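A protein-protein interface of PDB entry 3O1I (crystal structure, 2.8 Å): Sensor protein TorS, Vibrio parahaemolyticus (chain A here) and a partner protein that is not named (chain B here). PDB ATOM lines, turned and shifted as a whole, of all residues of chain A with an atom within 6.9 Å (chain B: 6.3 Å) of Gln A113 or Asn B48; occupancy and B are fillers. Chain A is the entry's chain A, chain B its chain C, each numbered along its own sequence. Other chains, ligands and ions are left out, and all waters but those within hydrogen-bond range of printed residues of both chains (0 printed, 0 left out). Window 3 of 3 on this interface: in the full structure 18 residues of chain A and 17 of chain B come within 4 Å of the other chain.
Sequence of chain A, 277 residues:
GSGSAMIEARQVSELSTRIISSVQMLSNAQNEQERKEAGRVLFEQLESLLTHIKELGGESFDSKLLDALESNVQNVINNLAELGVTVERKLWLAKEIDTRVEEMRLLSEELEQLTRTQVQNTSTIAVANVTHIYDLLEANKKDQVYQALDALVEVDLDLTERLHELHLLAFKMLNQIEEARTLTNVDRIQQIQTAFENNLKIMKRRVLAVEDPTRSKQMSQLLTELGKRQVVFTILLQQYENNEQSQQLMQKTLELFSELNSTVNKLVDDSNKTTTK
Of the 16 printed residues of chain A, 5 touch a printed residue of chain B.
Printed residues of chain A that touch a printed residue of chain B: Leu A106, Glu A109, Glu A110, Gln A113 and Thr A117.
Printed residues of chain B that touch a printed residue of chain A: Lys B16, Glu B42, Asn B48 and Arg B51.
Of the printed residues of chain B, Gln A113 touches Asn B48 and Arg B51.
Asn B48 touches just one residue of chain A: Gln A113 (2.8 Å).
Printed residues of chain B within 4 Å of Glu A110: Arg B51.
Printed residues of chain A within 4 Å of Arg B51: Leu A106 (3.3 Å), Glu A109 (3.7 Å), Glu A110 (3.3 Å) and Gln A113 (2.8 Å).
Of the printed residues of chain B, Leu A106 touches Arg B51 (3.3 Å).
Of the printed residues of chain A, Glu B42 touches Thr A117 (3.8 Å).
The nearest residue of chain A that does not touch Asn B48 is Glu A109 (6.2 Å).
The nearest printed residue of chain A that does not touch Glu B42 is Leu A114 (4.6 Å).
OG1 of Thr A117 lies within hydrogen-bond range of O of Leu A114 (2.6 Å).
The side-chain carboxylate of Glu B42 is in hydrogen-bond range of the backbone NH of Gly B44.
The backbone carbonyl oxygen (O) of Ala B43 sits at hydrogen-bond distance from the side-chain amide nitrogen (ND2) of Asn B48 (2.9 Å).
Among the printed residues, merely in contact across the chains: Glu A110 with Arg B51 (3.3 Å), Thr A117 with Lys B16 (3.6 Å) and Thr A117 with Glu B42 (3.8 Å).
O of Leu A106 is in hydrogen-bond range of NH2 of Arg B51, at 3.3 Å.
The side-chain carboxylate (OE1) of Glu A109 is in salt-bridge range of the guanidinium group (NH2) of Arg B51 (3.7 Å).
The side-chain amide oxygen (OE1) of Gln A113 lies within hydrogen-bond range of the side-chain amide nitrogen (ND2) of Asn B48 (2.8 Å).
The side-chain amide oxygen (OE1) of Gln A113 lies within hydrogen-bond range of the guanidinium group (NH1) of Arg B51.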
ATOM      1  N   LEU A 106      17.547  -4.755 -20.585  1.00  0.00           N
ATOM      2  CA  LEU A 106      17.023  -3.639 -19.814  1.00  0.00           C
ATOM      3  C   LEU A 106      15.563  -3.343 -20.094  1.00  0.00           C
ATOM      4  O   LEU A 106      14.774  -3.066 -19.174  1.00  0.00           O
ATOM      5  CB  LEU A 106      17.881  -2.380 -20.047  1.00  0.00           C
ATOM      6  CG  LEU A 106      19.316  -2.465 -19.476  1.00  0.00           C
ATOM      7  CD1 LEU A 106      20.068  -1.190 -19.775  1.00  0.00           C
ATOM      8  CD2 LEU A 106      19.282  -2.739 -17.962  1.00  0.00           C
ATOM      9  N   SER A 108      13.099  -5.469 -21.490  1.00  0.00           N
ATOM     10  CA  SER A 108      12.194  -6.537 -21.100  1.00  0.00           C
ATOM     11  C   SER A 108      12.189  -6.736 -19.603  1.00  0.00           C
ATOM     12  O   SER A 108      11.215  -7.230 -19.031  1.00  0.00           O
ATOM     13  CB  SER A 108      12.575  -7.843 -21.803  1.00  0.00           C
ATOM     14  OG  SER A 108      13.758  -8.375 -21.254  1.00  0.00           O
ATOM     15  N   GLU A 109      13.288  -6.363 -18.971  1.00  0.00           N
ATOM     16  CA  GLU A 109      13.393  -6.480 -17.529  1.00  0.00           C
ATOM     17  C   GLU A 109      12.438  -5.454 -16.915  1.00  0.00           C
ATOM     18  O   GLU A 109      11.732  -5.726 -15.944  1.00  0.00           O
ATOM     19  CB  GLU A 109      14.813  -6.180 -17.093  1.00  0.00           C
ATOM     20  CG  GLU A 109      15.033  -6.373 -15.631  1.00  0.00           C
ATOM     21  CD  GLU A 109      16.460  -6.097 -15.240  1.00  0.00           C
ATOM     22  OE1 GLU A 109      16.918  -4.933 -15.387  1.00  0.00           O
ATOM     23  OE2 GLU A 109      17.121  -7.055 -14.786  1.00  0.00           O
ATOM     24  N   GLU A 110      12.419  -4.266 -17.494  1.00  0.00           N
ATOM     25  CA  GLU A 110      11.547  -3.234 -17.006  1.00  0.00           C
ATOM     26  C   GLU A 110      10.104  -3.681 -17.193  1.00  0.00           C
ATOM     27  O   GLU A 110       9.271  -3.530 -16.301  1.00  0.00           O
ATOM     28  CB  GLU A 110      11.812  -1.952 -17.766  1.00  0.00           C
ATOM     29  CG  GLU A 110      10.913  -0.851 -17.375  1.00  0.00           C
ATOM     30  CD  GLU A 110      11.198   0.374 -18.156  1.00  0.00           C
ATOM     31  OE1 GLU A 110      11.113   0.303 -19.397  1.00  0.00           O
ATOM     32  OE2 GLU A 110      11.510   1.410 -17.532  1.00  0.00           O
ATOM     33  N   LEU A 111       9.815  -4.238 -18.359  1.00  0.00           N
ATOM     34  CA  LEU A 111       8.477  -4.716 -18.661  1.00  0.00           C
ATOM     35  C   LEU A 111       8.038  -5.802 -17.678  1.00  0.00           C
ATOM     36  O   LEU A 111       6.895  -5.839 -17.243  1.00  0.00           O
ATOM     37  CB  LEU A 111       8.426  -5.273 -20.083  1.00  0.00           C
ATOM     38  CG  LEU A 111       7.048  -5.821 -20.430  1.00  0.00           C
ATOM     39  CD1 LEU A 111       6.028  -4.697 -20.298  1.00  0.00           C
ATOM     40  CD2 LEU A 111       7.039  -6.392 -21.840  1.00  0.00           C
ATOM     41  N   GLU A 112       8.948  -6.694 -17.324  1.00  0.00           N
ATOM     42  CA  GLU A 112       8.588  -7.758 -16.406  1.00  0.00           C
ATOM     43  C   GLU A 112       8.267  -7.170 -15.029  1.00  0.00           C
ATOM     44  O   GLU A 112       7.294  -7.585 -14.383  1.00  0.00           O
ATOM     45  CB  GLU A 112       9.720  -8.792 -16.348  1.00  0.00           C
ATOM     46  CG  GLU A 112       9.514  -9.951 -15.387  1.00  0.00           C
ATOM     47  CD  GLU A 112       9.849  -9.572 -13.954  1.00  0.00           C
ATOM     48  OE1 GLU A 112      10.917  -8.959 -13.751  1.00  0.00           O
ATOM     49  OE2 GLU A 112       9.063  -9.890 -13.034  1.00  0.00           O
ATOM     50  N   GLN A 113       9.068  -6.188 -14.598  1.00  0.00           N
ATOM     51  CA  GLN A 113       8.871  -5.513 -13.307  1.00  0.00           C
ATOM     52  C   GLN A 113       7.583  -4.679 -13.324  1.00  0.00           C
ATOM     53  O   GLN A 113       6.908  -4.524 -12.308  1.00  0.00           O
ATOM     54  CB  GLN A 113      10.050  -4.589 -13.001  1.00  0.00           C
ATOM     55  CG  GLN A 113      11.401  -5.261 -13.054  1.00  0.00           C
ATOM     56  CD  GLN A 113      12.542  -4.315 -12.720  1.00  0.00           C
ATOM     57  OE1 GLN A 113      12.476  -3.111 -13.001  1.00  0.00           O
ATOM     58  NE2 GLN A 113      13.608  -4.857 -12.136  1.00  0.00           N
ATOM     59  N   LEU A 114       7.256  -4.131 -14.487  1.00  0.00           N
ATOM     60  CA  LEU A 114       6.060  -3.328 -14.625  1.00  0.00           C
ATOM     61  C   LEU A 114       4.840  -4.228 -14.414  1.00  0.00           C
ATOM     62  O   LEU A 114       3.978  -3.928 -13.599  1.00  0.00           O
ATOM     63  CB  LEU A 114       6.021  -2.667 -16.009  1.00  0.00           C
ATOM     64  CG  LEU A 114       4.921  -1.624 -16.262  1.00  0.00           C
ATOM     65  CD1 LEU A 114       5.065  -0.437 -15.329  1.00  0.00           C
ATOM     66  CD2 LEU A 114       5.010  -1.145 -17.687  1.00  0.00           C
ATOM     67  N   THR A 115       4.770  -5.329 -15.150  1.00  0.00           N
ATOM     68  CA  THR A 115       3.657  -6.258 -15.011  1.00  0.00           C
ATOM     69  C   THR A 115       3.602  -6.783 -13.575  1.00  0.00           C
ATOM     70  O   THR A 115       2.532  -7.076 -13.050  1.00  0.00           O
ATOM     71  CB  THR A 115       3.812  -7.485 -15.937  1.00  0.00           C
ATOM     72  OG1 THR A 115       5.084  -8.095 -15.695  1.00  0.00           O
ATOM     73  CG2 THR A 115       3.704  -7.099 -17.387  1.00  0.00           C
ATOM     74  N   ARG A 116       4.761  -6.922 -12.942  1.00  0.00           N
ATOM     75  CA  ARG A 116       4.793  -7.409 -11.571  1.00  0.00           C
ATOM     76  C   ARG A 116       4.104  -6.391 -10.673  1.00  0.00           C
ATOM     77  O   ARG A 116       3.206  -6.738  -9.919  1.00  0.00           O
ATOM     78  CB  ARG A 116       6.231  -7.623 -11.116  1.00  0.00           C
ATOM     79  CG  ARG A 116       6.353  -8.369  -9.811  1.00  0.00           C
ATOM     80  CD  ARG A 116       7.650  -9.158  -9.793  1.00  0.00           C
ATOM     81  NE  ARG A 116       7.488 -10.464  -9.154  1.00  0.00           N
ATOM     82  CZ  ARG A 116       8.325 -11.485  -9.332  1.00  0.00           C
ATOM     83  NH1 ARG A 116       9.386 -11.354 -10.131  1.00  0.00           N
ATOM     84  NH2 ARG A 116       8.105 -12.641  -8.714  1.00  0.00           N
ATOM     85  N   THR A 117       4.523  -5.132 -10.767  1.00  0.00           N
ATOM     86  CA  THR A 117       3.916  -4.075  -9.964  1.00  0.00           C
ATOM     87  C   THR A 117       2.395  -4.032 -10.163  1.00  0.00           C
ATOM     88  O   THR A 117       1.651  -3.819  -9.205  1.00  0.00           O
ATOM     89  CB  THR A 117       4.499  -2.666 -10.294  1.00  0.00           C
ATOM     90  OG1 THR A 117       4.159  -2.313 -11.633  1.00  0.00           O
ATOM     91  CG2 THR A 117       6.016  -2.655 -10.147  1.00  0.00           C
ATOM     92  N   GLN A 118       1.922  -4.242 -11.385  1.00  0.00           N
ATOM     93  CA  GLN A 118       0.490  -4.211 -11.611  1.00  0.00           C
ATOM     94  C   GLN A 118      -0.189  -5.348 -10.868  1.00  0.00           C
ATOM     95  O   GLN A 118      -1.285  -5.208 -10.334  1.00  0.00           O
ATOM     96  CB  GLN A 118       0.189  -4.299 -13.098  1.00  0.00           C
ATOM     97  CG  GLN A 118       0.712  -3.114 -13.872  1.00  0.00           C
ATOM     98  CD  GLN A 118       0.277  -3.136 -15.324  1.00  0.00           C
ATOM     99  OE1 GLN A 118      -0.897  -2.934 -15.635  1.00  0.00           O
ATOM    100  NE2 GLN A 118       1.227  -3.391 -16.224  1.00  0.00           N
ATOM    101  N   VAL A 119       0.484  -6.484 -10.839  1.00  0.00           N
ATOM    102  CA  VAL A 119      -0.032  -7.656 -10.161  1.00  0.00           C
ATOM    103  C   VAL A 119      -0.252  -7.340  -8.677  1.00  0.00           C
ATOM    104  O   VAL A 119      -1.325  -7.594  -8.119  1.00  0.00           O
ATOM    105  CB  VAL A 119       0.966  -8.852 -10.343  1.00  0.00           C
ATOM    106  CG1 VAL A 119       0.817  -9.873  -9.222  1.00  0.00           C
ATOM    107  CG2 VAL A 119       0.737  -9.507 -11.722  1.00  0.00           C
ATOM    108  N   HIS A 167       2.147 -11.429 -16.959  1.00  0.00           N
ATOM    109  CA  HIS A 167       3.398 -11.548 -16.248  1.00  0.00           C
ATOM    110  C   HIS A 167       4.197 -12.789 -16.643  1.00  0.00           C
ATOM    111  O   HIS A 167       5.435 -12.772 -16.594  1.00  0.00           O
ATOM    112  CB  HIS A 167       3.102 -11.558 -14.759  1.00  0.00           C
ATOM    113  CG  HIS A 167       4.300 -11.781 -13.905  1.00  0.00           C
ATOM    114  ND1 HIS A 167       5.429 -10.996 -13.986  1.00  0.00           N
ATOM    115  CD2 HIS A 167       4.519 -12.654 -12.896  1.00  0.00           C
ATOM    116  CE1 HIS A 167       6.291 -11.370 -13.059  1.00  0.00           C
ATOM    117  NE2 HIS A 167       5.762 -12.374 -12.383  1.00  0.00           N
ATOM    118  N   ALA A 170       5.739 -11.952 -20.098  1.00  0.00           N
ATOM    119  CA  ALA A 170       6.849 -11.025 -20.022  1.00  0.00           C
ATOM    120  C   ALA A 170       8.082 -11.736 -19.458  1.00  0.00           C
ATOM    121  O   ALA A 170       9.198 -11.484 -19.882  1.00  0.00           O
ATOM    122  CB  ALA A 170       6.467  -9.818 -19.155  1.00  0.00           C
ATOM    123  N   LEU A 174      11.648 -12.205 -21.215  1.00  0.00           N
ATOM    124  CA  LEU A 174      12.864 -11.826 -20.556  1.00  0.00           C
ATOM    125  C   LEU A 174      13.867 -12.988 -20.549  1.00  0.00           C
ATOM    126  O   LEU A 174      15.075 -12.768 -20.669  1.00  0.00           O
ATOM    127  CB  LEU A 174      12.550 -11.375 -19.133  1.00  0.00           C
ATOM    128  CG  LEU A 174      13.755 -11.156 -18.207  1.00  0.00           C
ATOM    129  CD1 LEU A 174      14.783 -10.218 -18.859  1.00  0.00           C
ATOM    130  CD2 LEU A 174      13.252 -10.594 -16.892  1.00  0.00           C
ATOM    131  N   PRO B  13      10.557   4.776  -5.211  1.00  0.00           N
ATOM    132  CA  PRO B  13      11.545   3.696  -5.323  1.00  0.00           C
ATOM    133  C   PRO B  13      10.840   2.515  -6.012  1.00  0.00           C
ATOM    134  O   PRO B  13      11.478   1.588  -6.504  1.00  0.00           O
ATOM    135  CB  PRO B  13      11.908   3.417  -3.873  1.00  0.00           C
ATOM    136  CG  PRO B  13      10.607   3.647  -3.171  1.00  0.00           C
ATOM    137  CD  PRO B  13      10.058   4.896  -3.828  1.00  0.00           C
ATOM    138  N   LYS B  16       4.616  -0.730  -5.458  1.00  0.00           N
ATOM    139  CA  LYS B  16       4.087  -2.063  -5.175  1.00  0.00           C
ATOM    140  C   LYS B  16       3.369  -2.166  -3.817  1.00  0.00           C
ATOM    141  O   LYS B  16       2.332  -2.821  -3.717  1.00  0.00           O
ATOM    142  CB  LYS B  16       5.226  -3.085  -5.256  1.00  0.00           C
ATOM    143  CG  LYS B  16       5.887  -3.127  -6.623  1.00  0.00           C
ATOM    144  CD  LYS B  16       7.021  -4.147  -6.720  1.00  0.00           C
ATOM    145  CE  LYS B  16       8.234  -3.731  -5.903  1.00  0.00           C
ATOM    146  NZ  LYS B  16       9.409  -4.611  -6.166  1.00  0.00           N
ATOM    147  N   GLU B  42       8.383   5.720 -11.219  1.00  0.00           N
ATOM    148  CA  GLU B  42       8.759   4.774 -10.182  1.00  0.00           C
ATOM    149  C   GLU B  42       9.873   3.865 -10.676  1.00  0.00           C
ATOM    150  O   GLU B  42       9.774   3.269 -11.750  1.00  0.00           O
ATOM    151  CB  GLU B  42       7.528   3.968  -9.743  1.00  0.00           C
ATOM    152  CG  GLU B  42       6.970   3.030 -10.791  1.00  0.00           C
ATOM    153  CD  GLU B  42       7.433   1.603 -10.587  1.00  0.00           C
ATOM    154  OE1 GLU B  42       7.117   0.753 -11.446  1.00  0.00           O
ATOM    155  OE2 GLU B  42       8.104   1.326  -9.562  1.00  0.00           O
ATOM    156  N   ALA B  43      10.932   3.768  -9.880  1.00  0.00           N
ATOM    157  CA  ALA B  43      12.105   2.966 -10.211  1.00  0.00           C
ATOM    158  C   ALA B  43      11.863   1.466 -10.360  1.00  0.00           C
ATOM    159  O   ALA B  43      12.800   0.705 -10.657  1.00  0.00           O
ATOM    160  CB  ALA B  43      13.182   3.198  -9.171  1.00  0.00           C
ATOM    161  N   GLY B  44      10.622   1.039 -10.146  1.00  0.00           N
ATOM    162  CA  GLY B  44      10.294  -0.369 -10.259  1.00  0.00           C
ATOM    163  C   GLY B  44      10.901  -1.280  -9.201  1.00  0.00           C
ATOM    164  O   GLY B  44      10.653  -2.481  -9.225  1.00  0.00           O
ATOM    165  N   GLY B  45      11.693  -0.744  -8.278  1.00  0.00           N
ATOM    166  CA  GLY B  45      12.276  -1.599  -7.260  1.00  0.00           C
ATOM    167  C   GLY B  45      13.412  -0.945  -6.504  1.00  0.00           C
ATOM    168  O   GLY B  45      14.055  -0.048  -7.024  1.00  0.00           O
ATOM    169  N   TYR B  46      13.668  -1.383  -5.276  1.00  0.00           N
ATOM    170  CA  TYR B  46      14.734  -0.779  -4.498  1.00  0.00           C
ATOM    171  C   TYR B  46      16.112  -1.075  -5.040  1.00  0.00           C
ATOM    172  O   TYR B  46      17.004  -0.228  -4.979  1.00  0.00           O
ATOM    173  CB  TYR B  46      14.658  -1.203  -3.025  1.00  0.00           C
ATOM    174  CG  TYR B  46      13.839  -0.245  -2.178  1.00  0.00           C
ATOM    175  CD1 TYR B  46      12.479  -0.059  -2.423  1.00  0.00           C
ATOM    176  CD2 TYR B  46      14.429   0.510  -1.169  1.00  0.00           C
ATOM    177  CE1 TYR B  46      11.726   0.854  -1.688  1.00  0.00           C
ATOM    178  CE2 TYR B  46      13.678   1.439  -0.424  1.00  0.00           C
ATOM    179  CZ  TYR B  46      12.327   1.600  -0.693  1.00  0.00           C
ATOM    180  OH  TYR B  46      11.569   2.493   0.027  1.00  0.00           O
ATOM    181  N   PRO B  47      16.317  -2.279  -5.587  1.00  0.00           N
ATOM    182  CA  PRO B  47      17.667  -2.532  -6.097  1.00  0.00           C
ATOM    183  C   PRO B  47      17.850  -1.928  -7.484  1.00  0.00           C
ATOM    184  O   PRO B  47      18.869  -2.148  -8.126  1.00  0.00           O
ATOM    185  CB  PRO B  47      17.756  -4.058  -6.116  1.00  0.00           C
ATOM    186  CG  PRO B  47      16.567  -4.528  -5.280  1.00  0.00           C
ATOM    187  CD  PRO B  47      15.515  -3.512  -5.601  1.00  0.00           C
ATOM    188  N   ASN B  48      16.861  -1.160  -7.935  1.00  0.00           N
ATOM    189  CA  ASN B  48      16.912  -0.532  -9.252  1.00  0.00           C
ATOM    190  C   ASN B  48      17.462   0.876  -9.207  1.00  0.00           C
ATOM    191  O   ASN B  48      16.831   1.815  -9.704  1.00  0.00           O
ATOM    192  CB  ASN B  48      15.523  -0.509  -9.881  1.00  0.00           C
ATOM    193  CG  ASN B  48      14.990  -1.886 -10.108  1.00  0.00           C
ATOM    194  OD1 ASN B  48      15.602  -2.866  -9.683  1.00  0.00           O
ATOM    195  ND2 ASN B  48      13.844  -1.986 -10.771  1.00  0.00           N
ATOM    196  N   LYS B  49      18.652   1.011  -8.631  1.00  0.00           N
ATOM    197  CA  LYS B  49      19.305   2.307  -8.501  1.00  0.00           C
ATOM    198  C   LYS B  49      19.608   2.924  -9.865  1.00  0.00           C
ATOM    199  O   LYS B  49      19.262   4.084 -10.135  1.00  0.00           O
ATOM    200  CB  LYS B  49      20.579   2.139  -7.663  1.00  0.00           C
ATOM    201  CG  LYS B  49      20.241   1.599  -6.263  1.00  0.00           C
ATOM    202  CD  LYS B  49      21.413   1.016  -5.492  1.00  0.00           C
ATOM    203  CE  LYS B  49      20.898   0.349  -4.212  1.00  0.00           C
ATOM    204  NZ  LYS B  49      22.001  -0.147  -3.331  1.00  0.00           N
ATOM    205  N   SER B  50      20.228   2.132 -10.733  1.00  0.00           N
ATOM    206  CA  SER B  50      20.573   2.596 -12.069  1.00  0.00           C
ATOM    207  C   SER B  50      19.359   3.188 -12.764  1.00  0.00           C
ATOM    208  O   SER B  50      19.457   4.210 -13.438  1.00  0.00           O
ATOM    209  CB  SER B  50      21.121   1.437 -12.903  1.00  0.00           C
ATOM    210  OG  SER B  50      22.133   0.743 -12.197  1.00  0.00           O
ATOM    211  N   ARG B  51      18.211   2.549 -12.588  1.00  0.00           N
ATOM    212  CA  ARG B  51      16.997   3.028 -13.224  1.00  0.00           C
ATOM    213  C   ARG B  51      16.475   4.341 -12.643  1.00  0.00           C
ATOM    214  O   ARG B  51      15.820   5.118 -13.342  1.00  0.00           O
ATOM    215  CB  ARG B  51      15.907   1.956 -13.156  1.00  0.00           C
ATOM    216  CG  ARG B  51      14.643   2.329 -13.911  1.00  0.00           C
ATOM    217  CD  ARG B  51      13.949   1.087 -14.405  1.00  0.00           C
ATOM    218  NE  ARG B  51      14.834   0.315 -15.269  1.00  0.00           N
ATOM    219  CZ  ARG B  51      14.649  -0.967 -15.570  1.00  0.00           C
ATOM    220  NH1 ARG B  51      13.603  -1.617 -15.068  1.00  0.00           N
ATOM    221  NH2 ARG B  51      15.508  -1.605 -16.365  1.00  0.00           N
ATOM    222  N   GLN B  52      16.761   4.598 -11.371  1.00  0.00           N
ATOM    223  CA  GLN B  52      16.294   5.836 -10.747  1.00  0.00           C
ATOM    224  C   GLN B  52      17.201   6.997 -11.161  1.00  0.00           C
ATOM    225  O   GLN B  52      16.716   8.101 -11.411  1.00  0.00           O
ATOM    226  CB  GLN B  52      16.243   5.700  -9.212  1.00  0.00           C
ATOM    227  CG  GLN B  52      15.489   6.848  -8.526  1.00  0.00           C
ATOM    228  CD  GLN B  52      15.377   6.703  -7.011  1.00  0.00           C
ATOM    229  OE1 GLN B  52      16.376   6.500  -6.320  1.00  0.00           O
ATOM    230  NE2 GLN B  52      14.155   6.821  -6.492  1.00  0.00           N
ATOM    231  N   GLU B  53      18.508   6.737 -11.240  1.00  0.00           N
ATOM    232  CA  GLU B  53      19.481   7.747 -11.664  1.00  0.00           C
ATOM    233  C   GLU B  53      19.049   8.271 -13.020  1.00  0.00           C
ATOM    234  O   GLU B  53      19.091   9.468 -13.275  1.00  0.00           O
ATOM    235  CB  GLU B  53      20.876   7.142 -11.794  1.00  0.00           C
ATOM    236  CG  GLU B  53      21.480   6.685 -10.494  1.00  0.00           C
ATOM    237  CD  GLU B  53      22.844   6.067 -10.688  1.00  0.00           C
ATOM    238  OE1 GLU B  53      22.949   5.122 -11.497  1.00  0.00           O
ATOM    239  OE2 GLU B  53      23.809   6.519 -10.036  1.00  0.00           O
ATOM    240  N   VAL B  72      16.031   5.116  -3.289  1.00  0.00           N
ATOM    241  CA  VAL B  72      16.156   3.676  -3.153  1.00  0.00           C
ATOM    242  C   VAL B  72      17.422   3.446  -2.357  1.00  0.00           C
ATOM    243  O   VAL B  72      18.021   2.385  -2.414  1.00  0.00           O
ATOM    244  CB  VAL B  72      16.300   3.007  -4.547  1.00  0.00           C
ATOM    245  CG1 VAL B  72      15.082   3.339  -5.410  1.00  0.00           C
ATOM    246  CG2 VAL B  72      17.583   3.484  -5.230  1.00  0.00           C
